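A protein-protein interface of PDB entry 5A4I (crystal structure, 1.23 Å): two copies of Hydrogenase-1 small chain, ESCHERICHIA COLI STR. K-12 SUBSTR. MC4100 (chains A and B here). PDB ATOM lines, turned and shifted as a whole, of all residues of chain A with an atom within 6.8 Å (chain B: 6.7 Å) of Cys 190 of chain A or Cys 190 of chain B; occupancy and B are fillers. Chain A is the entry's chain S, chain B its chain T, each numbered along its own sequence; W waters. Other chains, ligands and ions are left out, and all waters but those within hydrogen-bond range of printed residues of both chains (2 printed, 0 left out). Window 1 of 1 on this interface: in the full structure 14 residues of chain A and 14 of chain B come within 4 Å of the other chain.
Of chain B, only Cys 190 and Tyr 191 come within 4 Å of Cys 190 of chain A. Of the printed residues of chain B, Asp 188 of chain A touches Tyr 191 (3.997 Å) and Ala 194 (3.3 Å). Of the printed residues of chain A, Lys 189 of chain B touches Tyr 191. Of the printed residues of chain B, His 187 of chain A touches Ala 194. Of the printed residues of chain A, Tyr 191 of chain B touches Asp 188 (3.997 Å), Lys 189 (3.2 Å), Cys 190 (3.9 Å), Tyr 191 (3.9 Å) and Ser 232 (3.9 Å). Arg 185 of chain B touches none of the printed residues of chain A. The nearest residue of chain B that does not touch Cys 190 of chain A is Arg 193 of chain B (5.2 Å). The nearest printed residue of chain A that does not touch His 187 of chain B is Tyr 191 of chain A (6.3 Å).
Hydrophobic or aromatic side chains of chain A within 4 Å of the printed part of chain B: Tyr 191 and Ala 194. Hydrophobic or aromatic side chains of chain B that line the printed part of chain A: Tyr 191 and Ala 194. Among the printed residues, 16 pairs touch across the chains.
Water W2 lies within hydrogen-bond range of the backbone carbonyl oxygen (O) of Tyr 191 of chain B (2.8 Å), the backbone NH (N) of Ala 194 of chain B (2.9 Å), the backbone carbonyl oxygen (O) of Cys 190 of chain A (2.9 Å) and the backbone NH (N) of Arg 193 of chain B (3.4 Å). Water W1 lies within hydrogen-bond range of the backbone carbonyl oxygen of Tyr 191 of chain A (2.8 Å), the backbone carbonyl oxygen of Cys 190 of chain B (2.9 Å), the backbone NH of Ala 194 of chain A (2.9 Å) and the backbone NH of Arg 193 of chain A (3.4 Å).
CB of Ala 194 of chain B touches O of His 187 of chain A, at 3.8 Å. Asp 188 of chain A touches Tyr 191 of chain B (O to O, 3.997 Å). Asp 188 of chain A touches Ala 194 of chain B. Lys 189 of chain A touches Tyr 191 of chain B (CA to O, 3.2 Å). Cys 190 of chain A touches Cys 190 of chain B (O to O, 3.9 Å). Ser 232 of chain B touches Tyr 191 of chain A. Arg 193 of chain A touches Ala 194 of chain B. Ala 194 of chain A touches His 187 of chain B. Arg 193 of chain B touches Ala 194 of chain A (NH1 to CB, 3.2 Å). Tyr 191 of chain B touches Ser 232 of chain A.
His 187 of chain A touches Ala 194 of chain B, and with the chains exchanged Ala 194 of chain A touches His 187 of chain B. Asp 188 of chain A touches Ala 194 of chain B, and with the chains exchanged Ala 194 of chain A touches Asp 188 of chain B. Tyr 191 of chain B touches its own counterpart, Tyr 191 of chain A. Tyr 191 of chain A touches Ser 232 of chain B, and with the chains exchanged Ser 232 of chain A touches Tyr 191 of chain B. Positions printed for both chains: 185, 186, 187, 188, 189, 190, 191, 192, 193, 194, 221, 231, 232, 241 and 243.
The backbone NH (N) of Arg 192 of chain B lies close to the side-chain sulfur (SG) of Cys 190 of chain B (3.4 Å). OG of Ser 231 of chain A lies close to O of Lys 189 of chain A (3.3 Å). The backbone NH (N) of Arg 192 of chain A sits close to the side-chain sulfur (SG) of Cys 190 of chain A, at 3.4 Å. The guanidinium group (NH1) of Arg 185 of chain B is in salt-bridge range of the side-chain carboxylate (OD2) of Asp 188 of chain B (3.0 Å). The backbone carbonyl oxygen (O) of Lys 189 of chain B lies close to the side-chain hydroxyl (OG) of Ser 231 of chain B. The side-chain hydroxyl (OH) of Tyr 191 of chain A sits at hydrogen-bond distance from the guanidinium group (NH2) of Arg 192 of chain A (3.1 Å).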
ATOM      1  N   ARG A 185      -3.987 -19.833  29.229  1.00  0.00           N
ATOM      2  CA  ARG A 185      -4.423 -19.055  28.091  1.00  0.00           C
ATOM      3  C   ARG A 185      -5.380 -19.874  27.220  1.00  0.00           C
ATOM      4  O   ARG A 185      -5.290 -21.118  27.119  1.00  0.00           O
ATOM      5  CB  ARG A 185      -3.221 -18.637  27.244  1.00  0.00           C
ATOM      6  CG  ARG A 185      -2.247 -17.736  28.000  1.00  0.00           C
ATOM      7  CD  ARG A 185      -1.088 -17.449  27.029  1.00  0.00           C
ATOM      8  NE  ARG A 185       0.098 -16.929  27.640  1.00  0.00           N
ATOM      9  CZ  ARG A 185       1.149 -17.638  28.063  1.00  0.00           C
ATOM     10  NH1 ARG A 185       1.246 -18.979  27.950  1.00  0.00           N
ATOM     11  NH2 ARG A 185       2.131 -16.975  28.631  1.00  0.00           N
ATOM     12  N   ILE A 186      -6.257 -19.177  26.522  1.00  0.00           N
ATOM     13  CA  ILE A 186      -7.135 -19.782  25.538  1.00  0.00           C
ATOM     14  C   ILE A 186      -6.332 -20.645  24.568  1.00  0.00           C
ATOM     15  O   ILE A 186      -6.687 -21.791  24.273  1.00  0.00           O
ATOM     16  CB  ILE A 186      -7.969 -18.699  24.755  1.00  0.00           C
ATOM     17  CG1 ILE A 186      -8.962 -17.969  25.656  1.00  0.00           C
ATOM     18  CG2 ILE A 186      -8.630 -19.300  23.539  1.00  0.00           C
ATOM     19  CD1 ILE A 186     -10.087 -18.788  26.151  1.00  0.00           C
ATOM     20  N   HIS A 187      -5.265 -20.075  24.058  1.00  0.00           N
ATOM     21  CA  HIS A 187      -4.387 -20.722  23.042  1.00  0.00           C
ATOM     22  C   HIS A 187      -3.649 -21.940  23.569  1.00  0.00           C
ATOM     23  O   HIS A 187      -3.191 -22.719  22.741  1.00  0.00           O
ATOM     24  CB  HIS A 187      -3.446 -19.598  22.568  1.00  0.00           C
ATOM     25  CG  HIS A 187      -2.392 -19.916  21.568  1.00  0.00           C
ATOM     26  ND1 HIS A 187      -2.646 -20.071  20.234  1.00  0.00           N
ATOM     27  CD2 HIS A 187      -1.043 -19.907  21.689  1.00  0.00           C
ATOM     28  CE1 HIS A 187      -1.512 -20.223  19.573  1.00  0.00           C
ATOM     29  NE2 HIS A 187      -0.514 -20.131  20.438  1.00  0.00           N
ATOM     30  N   ASP A 188      -3.505 -22.077  24.886  1.00  0.00           N
ATOM     31  CA  ASP A 188      -2.871 -23.242  25.457  1.00  0.00           C
ATOM     32  C   ASP A 188      -3.784 -24.435  25.649  1.00  0.00           C
ATOM     33  O   ASP A 188      -3.306 -25.498  26.001  1.00  0.00           O
ATOM     34  CB  ASP A 188      -2.115 -22.824  26.679  1.00  0.00           C
ATOM     35  CG  ASP A 188      -0.871 -21.902  26.280  1.00  0.00           C
ATOM     36  OD1 ASP A 188      -0.321 -21.951  25.112  1.00  0.00           O
ATOM     37  OD2 ASP A 188      -0.410 -21.167  27.094  1.00  0.00           O
ATOM     38  N   LYS A 189      -5.081 -24.249  25.326  1.00  0.00           N
ATOM     39  CA  LYS A 189      -6.081 -25.335  25.366  1.00  0.00           C
ATOM     40  C   LYS A 189      -6.994 -25.247  24.155  1.00  0.00           C
ATOM     41  O   LYS A 189      -8.129 -25.715  24.188  1.00  0.00           O
ATOM     42  CB  LYS A 189      -6.898 -25.332  26.697  1.00  0.00           C
ATOM     43  CG  LYS A 189      -6.118 -25.889  27.868  1.00  0.00           C
ATOM     44  CD  LYS A 189      -5.760 -27.352  27.703  1.00  0.00           C
ATOM     45  CE  LYS A 189      -5.558 -28.117  28.992  1.00  0.00           C
ATOM     46  NZ  LYS A 189      -4.441 -27.589  29.808  1.00  0.00           N
ATOM     47  N   CYS A 190      -6.483 -24.711  23.032  1.00  0.00           N
ATOM     48  CA  CYS A 190      -7.328 -24.529  21.866  1.00  0.00           C
ATOM     49  C   CYS A 190      -7.210 -25.725  20.947  1.00  0.00           C
ATOM     50  O   CYS A 190      -6.118 -26.134  20.522  1.00  0.00           O
ATOM     51  CB  CYS A 190      -6.910 -23.301  21.100  1.00  0.00           C
ATOM     52  SG  CYS A 190      -7.972 -22.939  19.633  1.00  0.00           S
ATOM     53  N   TYR A 191      -8.368 -26.232  20.519  1.00  0.00           N
ATOM     54  CA  TYR A 191      -8.419 -27.393  19.623  1.00  0.00           C
ATOM     55  C   TYR A 191      -7.942 -27.107  18.216  1.00  0.00           C
ATOM     56  O   TYR A 191      -7.734 -28.053  17.484  1.00  0.00           O
ATOM     57  CB  TYR A 191      -9.842 -28.018  19.639  1.00  0.00           C
ATOM     58  CG  TYR A 191     -10.828 -27.367  18.699  1.00  0.00           C
ATOM     59  CD1 TYR A 191     -11.136 -25.990  18.744  1.00  0.00           C
ATOM     60  CD2 TYR A 191     -11.531 -28.126  17.757  1.00  0.00           C
ATOM     61  CE1 TYR A 191     -12.054 -25.433  17.879  1.00  0.00           C
ATOM     62  CE2 TYR A 191     -12.422 -27.555  16.876  1.00  0.00           C
ATOM     63  CZ  TYR A 191     -12.662 -26.199  16.919  1.00  0.00           C
ATOM     64  OH  TYR A 191     -13.487 -25.587  16.004  1.00  0.00           O
ATOM     65  N   ARG A 192      -7.696 -25.840  17.849  1.00  0.00           N
ATOM     66  CA  ARG A 192      -7.101 -25.517  16.564  1.00  0.00           C
ATOM     67  C   ARG A 192      -5.587 -25.342  16.639  1.00  0.00           C
ATOM     68  O   ARG A 192      -4.956 -25.008  15.615  1.00  0.00           O
ATOM     69  CB  ARG A 192      -7.773 -24.316  15.900  1.00  0.00           C
ATOM     70  CG  ARG A 192      -9.253 -24.551  15.663  1.00  0.00           C
ATOM     71  CD  ARG A 192      -9.914 -23.427  14.896  1.00  0.00           C
ATOM     72  NE  ARG A 192     -11.343 -23.638  14.739  1.00  0.00           N
ATOM     73  CZ  ARG A 192     -12.112 -23.138  13.788  1.00  0.00           C
ATOM     74  NH1 ARG A 192     -11.631 -22.341  12.844  1.00  0.00           N
ATOM     75  NH2 ARG A 192     -13.425 -23.412  13.800  1.00  0.00           N
ATOM     76  N   ARG A 193      -4.983 -25.634  17.779  1.00  0.00           N
ATOM     77  CA  ARG A 193      -3.550 -25.399  17.931  1.00  0.00           C
ATOM     78  C   ARG A 193      -2.714 -26.261  16.991  1.00  0.00           C
ATOM     79  O   ARG A 193      -1.685 -25.786  16.528  1.00  0.00           O
ATOM     80  CB  ARG A 193      -3.151 -25.647  19.345  1.00  0.00           C
ATOM     81  CG  ARG A 193      -1.740 -25.315  19.709  1.00  0.00           C
ATOM     82  CD  ARG A 193      -1.393 -23.825  19.568  1.00  0.00           C
ATOM     83  NE  ARG A 193       0.010 -23.771  19.913  1.00  0.00           N
ATOM     84  CZ  ARG A 193       0.515 -23.487  21.087  1.00  0.00           C
ATOM     85  NH1 ARG A 193      -0.222 -23.037  22.095  1.00  0.00           N
ATOM     86  NH2 ARG A 193       1.810 -23.629  21.243  1.00  0.00           N
ATOM     87  N   ALA A 194      -3.161 -27.460  16.644  1.00  0.00           N
ATOM     88  CA  ALA A 194      -2.470 -28.262  15.628  1.00  0.00           C
ATOM     89  C   ALA A 194      -2.263 -27.455  14.364  1.00  0.00           C
ATOM     90  O   ALA A 194      -1.216 -27.547  13.708  1.00  0.00           O
ATOM     91  CB  ALA A 194      -3.271 -29.505  15.316  1.00  0.00           C
ATOM     92  N   CYS A 221      -7.094 -13.537  15.849  1.00  0.00           N
ATOM     93  CA  CYS A 221      -7.392 -14.205  17.110  1.00  0.00           C
ATOM     94  C   CYS A 221      -6.444 -13.751  18.214  1.00  0.00           C
ATOM     95  O   CYS A 221      -5.220 -13.833  18.058  1.00  0.00           O
ATOM     96  CB  CYS A 221      -7.226 -15.725  16.948  1.00  0.00           C
ATOM     97  SG  CYS A 221      -7.724 -16.628  18.410  1.00  0.00           S
ATOM     98  N   SER A 231     -11.877 -22.322  25.765  1.00  0.00           N
ATOM     99  CA  SER A 231     -11.487 -23.419  24.895  1.00  0.00           C
ATOM    100  C   SER A 231     -11.546 -24.790  25.545  1.00  0.00           C
ATOM    101  O   SER A 231     -11.337 -25.792  24.875  1.00  0.00           O
ATOM    102  CB  SER A 231     -10.085 -23.156  24.315  1.00  0.00           C
ATOM    103  OG  SER A 231      -9.180 -22.816  25.371  1.00  0.00           O
ATOM    104  N   SER A 232     -11.895 -24.828  26.831  1.00  0.00           N
ATOM    105  CA  SER A 232     -11.958 -26.062  27.619  1.00  0.00           C
ATOM    106  C   SER A 232     -13.387 -26.287  28.119  1.00  0.00           C
ATOM    107  O   SER A 232     -14.113 -27.195  27.704  1.00  0.00           O
ATOM    108  CB  SER A 232     -11.017 -25.927  28.853  1.00  0.00           C
ATOM    109  OG  SER A 232      -9.647 -26.058  28.539  1.00  0.00           O
ATOM    110  N   PHE A 241     -17.637 -22.101  21.426  1.00  0.00           N
ATOM    111  CA  PHE A 241     -16.943 -20.921  21.912  1.00  0.00           C
ATOM    112  C   PHE A 241     -16.605 -20.106  20.673  1.00  0.00           C
ATOM    113  O   PHE A 241     -16.752 -20.601  19.547  1.00  0.00           O
ATOM    114  CB  PHE A 241     -15.766 -21.232  22.837  1.00  0.00           C
ATOM    115  CG  PHE A 241     -14.507 -21.774  22.200  1.00  0.00           C
ATOM    116  CD1 PHE A 241     -14.418 -23.046  21.698  1.00  0.00           C
ATOM    117  CD2 PHE A 241     -13.334 -21.001  22.291  1.00  0.00           C
ATOM    118  CE1 PHE A 241     -13.198 -23.530  21.200  1.00  0.00           C
ATOM    119  CE2 PHE A 241     -12.156 -21.491  21.803  1.00  0.00           C
ATOM    120  CZ  PHE A 241     -12.088 -22.750  21.262  1.00  0.00           C
ATOM    121  N   ILE A 243     -14.006 -19.252  18.838  1.00  0.00           N
ATOM    122  CA  ILE A 243     -13.138 -19.869  17.844  1.00  0.00           C
ATOM    123  C   ILE A 243     -13.810 -21.078  17.198  1.00  0.00           C
ATOM    124  O   ILE A 243     -13.693 -21.261  15.968  1.00  0.00           O
ATOM    125  CB  ILE A 243     -11.786 -20.223  18.504  1.00  0.00           C
ATOM    126  CG1 ILE A 243     -10.983 -18.951  18.783  1.00  0.00           C
ATOM    127  CG2 ILE A 243     -10.986 -21.218  17.686  1.00  0.00           C
ATOM    128  CD1 ILE A 243     -10.095 -19.035  19.991  1.00  0.00           C
ATOM    129  N   ARG B 185      -7.486 -36.324  11.914  1.00  0.00           N
ATOM    130  CA  ARG B 185      -7.025 -37.054  13.072  1.00  0.00           C
ATOM    131  C   ARG B 185      -7.464 -36.414  14.385  1.00  0.00           C
ATOM    132  O   ARG B 185      -7.622 -35.176  14.483  1.00  0.00           O
ATOM    133  CB  ARG B 185      -5.510 -37.234  13.039  1.00  0.00           C
ATOM    134  CG  ARG B 185      -4.995 -37.981  11.815  1.00  0.00           C
ATOM    135  CD  ARG B 185      -3.472 -37.908  11.865  1.00  0.00           C
ATOM    136  NE  ARG B 185      -2.770 -38.240  10.633  1.00  0.00           N
ATOM    137  CZ  ARG B 185      -2.267 -37.359   9.771  1.00  0.00           C
ATOM    138  NH1 ARG B 185      -2.414 -36.048   9.953  1.00  0.00           N
ATOM    139  NH2 ARG B 185      -1.641 -37.790   8.700  1.00  0.00           N
ATOM    140  N   ILE B 186      -7.606 -37.235  15.406  1.00  0.00           N
ATOM    141  CA  ILE B 186      -7.894 -36.739  16.763  1.00  0.00           C
ATOM    142  C   ILE B 186      -6.889 -35.666  17.160  1.00  0.00           C
ATOM    143  O   ILE B 186      -7.240 -34.604  17.672  1.00  0.00           O
ATOM    144  CB  ILE B 186      -7.853 -37.928  17.779  1.00  0.00           C
ATOM    145  CG1 ILE B 186      -9.002 -38.926  17.544  1.00  0.00           C
ATOM    146  CG2 ILE B 186      -7.852 -37.462  19.219  1.00  0.00           C
ATOM    147  CD1 ILE B 186     -10.354 -38.343  17.755  1.00  0.00           C
ATOM    148  N   HIS B 187      -5.619 -35.972  16.909  1.00  0.00           N
ATOM    149  CA  HIS B 187      -4.478 -35.104  17.271  1.00  0.00           C
ATOM    150  C   HIS B 187      -4.456 -33.807  16.499  1.00  0.00           C
ATOM    151  O   HIS B 187      -3.785 -32.879  16.940  1.00  0.00           O
ATOM    152  CB  HIS B 187      -3.232 -35.949  17.074  1.00  0.00           C
ATOM    153  CG  HIS B 187      -1.905 -35.334  17.337  1.00  0.00           C
ATOM    154  ND1 HIS B 187      -1.363 -35.172  18.604  1.00  0.00           N
ATOM    155  CD2 HIS B 187      -0.904 -35.068  16.465  1.00  0.00           C
ATOM    156  CE1 HIS B 187      -0.117 -34.752  18.491  1.00  0.00           C
ATOM    157  NE2 HIS B 187       0.185 -34.698  17.199  1.00  0.00           N
ATOM    158  N   ASP B 188      -5.151 -33.740  15.355  1.00  0.00           N
ATOM    159  CA  ASP B 188      -5.204 -32.489  14.603  1.00  0.00           C
ATOM    160  C   ASP B 188      -6.275 -31.533  15.088  1.00  0.00           C
ATOM    161  O   ASP B 188      -6.326 -30.409  14.587  1.00  0.00           O
ATOM    162  CB  ASP B 188      -5.159 -32.769  13.146  1.00  0.00           C
ATOM    163  CG  ASP B 188      -3.717 -33.364  12.762  1.00  0.00           C
ATOM    164  OD1 ASP B 188      -2.623 -33.089  13.417  1.00  0.00           O
ATOM    165  OD2 ASP B 188      -3.684 -34.089  11.875  1.00  0.00           O
ATOM    166  N   LYS B 189      -7.105 -31.968  16.030  1.00  0.00           N
ATOM    167  CA  LYS B 189      -8.122 -31.114  16.652  1.00  0.00           C
ATOM    168  C   LYS B 189      -8.148 -31.310  18.151  1.00  0.00           C
ATOM    169  O   LYS B 189      -9.163 -31.086  18.797  1.00  0.00           O
ATOM    170  CB  LYS B 189      -9.528 -31.404  16.039  1.00  0.00           C
ATOM    171  CG  LYS B 189      -9.732 -30.774  14.666  1.00  0.00           C
ATOM    172  CD  LYS B 189      -9.653 -29.262  14.722  1.00  0.00           C
ATOM    173  CE  LYS B 189     -10.418 -28.575  13.590  1.00  0.00           C
ATOM    174  NZ  LYS B 189      -9.867 -28.835  12.236  1.00  0.00           N
ATOM    175  N   CYS B 190      -7.007 -31.652  18.750  1.00  0.00           N
ATOM    176  CA  CYS B 190      -6.970 -31.949  20.167  1.00  0.00           C
ATOM    177  C   CYS B 190      -6.622 -30.672  20.931  1.00  0.00           C
ATOM    178  O   CYS B 190      -5.600 -30.005  20.695  1.00  0.00           O
ATOM    179  CB  CYS B 190      -5.908 -33.004  20.484  1.00  0.00           C
ATOM    180  SG  CYS B 190      -5.873 -33.471  22.272  1.00  0.00           S
ATOM    181  N   TYR B 191      -7.410 -30.385  21.967  1.00  0.00           N
ATOM    182  CA  TYR B 191      -7.190 -29.222  22.830  1.00  0.00           C
ATOM    183  C   TYR B 191      -5.938 -29.291  23.671  1.00  0.00           C
ATOM    184  O   TYR B 191      -5.545 -28.288  24.219  1.00  0.00           O
ATOM    185  CB  TYR B 191      -8.441 -28.897  23.650  1.00  0.00           C
ATOM    186  CG  TYR B 191      -8.598 -29.674  24.929  1.00  0.00           C
ATOM    187  CD1 TYR B 191      -8.544 -31.067  24.989  1.00  0.00           C
ATOM    188  CD2 TYR B 191      -8.779 -29.013  26.098  1.00  0.00           C
ATOM    189  CE1 TYR B 191      -8.643 -31.732  26.175  1.00  0.00           C
ATOM    190  CE2 TYR B 191      -8.888 -29.662  27.302  1.00  0.00           C
ATOM    191  CZ  TYR B 191      -8.810 -31.039  27.343  1.00  0.00           C
ATOM    192  OH  TYR B 191      -8.805 -31.731  28.542  1.00  0.00           O
ATOM    193  N   ARG B 192      -5.272 -30.443  23.741  1.00  0.00           N
ATOM    194  CA  ARG B 192      -4.001 -30.528  24.468  1.00  0.00           C
ATOM    195  C   ARG B 192      -2.808 -30.384  23.540  1.00  0.00           C
ATOM    196  O   ARG B 192      -1.666 -30.539  24.003  1.00  0.00           O
ATOM    197  CB  ARG B 192      -3.890 -31.822  25.316  1.00  0.00           C
ATOM    198  CG  ARG B 192      -4.994 -31.917  26.354  1.00  0.00           C
ATOM    199  CD  ARG B 192      -4.824 -33.077  27.286  1.00  0.00           C
ATOM    200  NE  ARG B 192      -5.956 -33.142  28.243  1.00  0.00           N
ATOM    201  CZ  ARG B 192      -5.931 -33.761  29.407  1.00  0.00           C
ATOM    202  NH1 ARG B 192      -4.829 -34.324  29.890  1.00  0.00           N
ATOM    203  NH2 ARG B 192      -7.018 -33.753  30.147  1.00  0.00           N
ATOM    204  N   ARG B 193      -3.030 -30.082  22.275  1.00  0.00           N
ATOM    205  CA  ARG B 193      -1.926 -30.016  21.298  1.00  0.00           C
ATOM    206  C   ARG B 193      -0.902 -28.942  21.693  1.00  0.00           C
ATOM    207  O   ARG B 193       0.279 -29.129  21.439  1.00  0.00           O
ATOM    208  CB  ARG B 193      -2.449 -29.789  19.927  1.00  0.00           C
ATOM    209  CG  ARG B 193      -1.438 -29.821  18.824  1.00  0.00           C
ATOM    210  CD  ARG B 193      -0.825 -31.222  18.634  1.00  0.00           C
ATOM    211  NE  ARG B 193       0.105 -31.000  17.583  1.00  0.00           N
ATOM    212  CZ  ARG B 193      -0.093 -31.237  16.309  1.00  0.00           C
ATOM    213  NH1 ARG B 193      -1.129 -31.872  15.836  1.00  0.00           N
ATOM    214  NH2 ARG B 193       0.805 -30.804  15.476  1.00  0.00           N
ATOM    215  N   ALA B 194      -1.321 -27.851  22.317  1.00  0.00           N
ATOM    216  CA  ALA B 194      -0.345 -26.837  22.800  1.00  0.00           C
ATOM    217  C   ALA B 194       0.709 -27.483  23.641  1.00  0.00           C
ATOM    218  O   ALA B 194       1.883 -27.118  23.631  1.00  0.00           O
ATOM    219  CB  ALA B 194      -1.053 -25.761  23.570  1.00  0.00           C
ATOM    220  N   CYS B 221      -1.043 -42.200  24.289  1.00  0.00           N
ATOM    221  CA  CYS B 221      -2.130 -41.694  23.439  1.00  0.00           C
ATOM    222  C   CYS B 221      -1.899 -41.999  21.959  1.00  0.00           C
ATOM    223  O   CYS B 221      -0.867 -41.665  21.395  1.00  0.00           O
ATOM    224  CB  CYS B 221      -2.226 -40.176  23.651  1.00  0.00           C
ATOM    225  SG  CYS B 221      -3.642 -39.468  22.718  1.00  0.00           S
ATOM    226  N   SER B 231     -12.335 -35.287  19.384  1.00  0.00           N
ATOM    227  CA  SER B 231     -11.728 -34.073  19.939  1.00  0.00           C
ATOM    228  C   SER B 231     -12.457 -32.810  19.520  1.00  0.00           C
ATOM    229  O   SER B 231     -12.112 -31.737  19.993  1.00  0.00           O
ATOM    230  CB  SER B 231     -10.238 -34.006  19.599  1.00  0.00           C
ATOM    231  OG  SER B 231     -10.045 -34.208  18.188  1.00  0.00           O
ATOM    232  N   SER B 232     -13.468 -32.925  18.663  1.00  0.00           N
ATOM    233  CA  SER B 232     -14.240 -31.771  18.143  1.00  0.00           C
ATOM    234  C   SER B 232     -15.724 -31.910  18.521  1.00  0.00           C
ATOM    235  O   SER B 232     -16.270 -31.158  19.288  1.00  0.00           O
ATOM    236  CB  SER B 232     -14.111 -31.692  16.603  1.00  0.00           C
ATOM    237  OG  SER B 232     -12.824 -31.393  16.111  1.00  0.00           O
ATOM    238  N   PHE B 241     -14.439 -36.386  26.187  1.00  0.00           N
ATOM    239  CA  PHE B 241     -13.893 -37.421  25.337  1.00  0.00           C
ATOM    240  C   PHE B 241     -12.740 -38.078  26.111  1.00  0.00           C
ATOM    241  O   PHE B 241     -12.328 -37.541  27.149  1.00  0.00           O
ATOM    242  CB  PHE B 241     -13.533 -36.937  23.909  1.00  0.00           C
ATOM    243  CG  PHE B 241     -12.271 -36.135  23.729  1.00  0.00           C
ATOM    244  CD1 PHE B 241     -12.179 -34.852  24.214  1.00  0.00           C
ATOM    245  CD2 PHE B 241     -11.224 -36.632  22.956  1.00  0.00           C
ATOM    246  CE1 PHE B 241     -11.025 -34.073  23.983  1.00  0.00           C
ATOM    247  CE2 PHE B 241     -10.121 -35.838  22.704  1.00  0.00           C
ATOM    248  CZ  PHE B 241     -10.022 -34.581  23.216  1.00  0.00           C
ATOM    249  N   ILE B 243      -9.446 -38.243  26.084  1.00  0.00           N
ATOM    250  CA  ILE B 243      -8.317 -37.372  26.461  1.00  0.00           C
ATOM    251  C   ILE B 243      -8.733 -36.329  27.458  1.00  0.00           C
ATOM    252  O   ILE B 243      -7.985 -36.030  28.401  1.00  0.00           O
ATOM    253  CB  ILE B 243      -7.719 -36.802  25.169  1.00  0.00           C
ATOM    254  CG1 ILE B 243      -6.940 -37.900  24.414  1.00  0.00           C
ATOM    255  CG2 ILE B 243      -6.809 -35.618  25.425  1.00  0.00           C
ATOM    256  CD1 ILE B 243      -6.973 -37.736  22.928  1.00  0.00           C
HETATM  257  O   HOH W   1      -5.166 -29.035  18.034  1.00  0.00           O
HETATM  258  O   HOH W   2      -4.007 -26.816  22.400  1.00  0.00           O
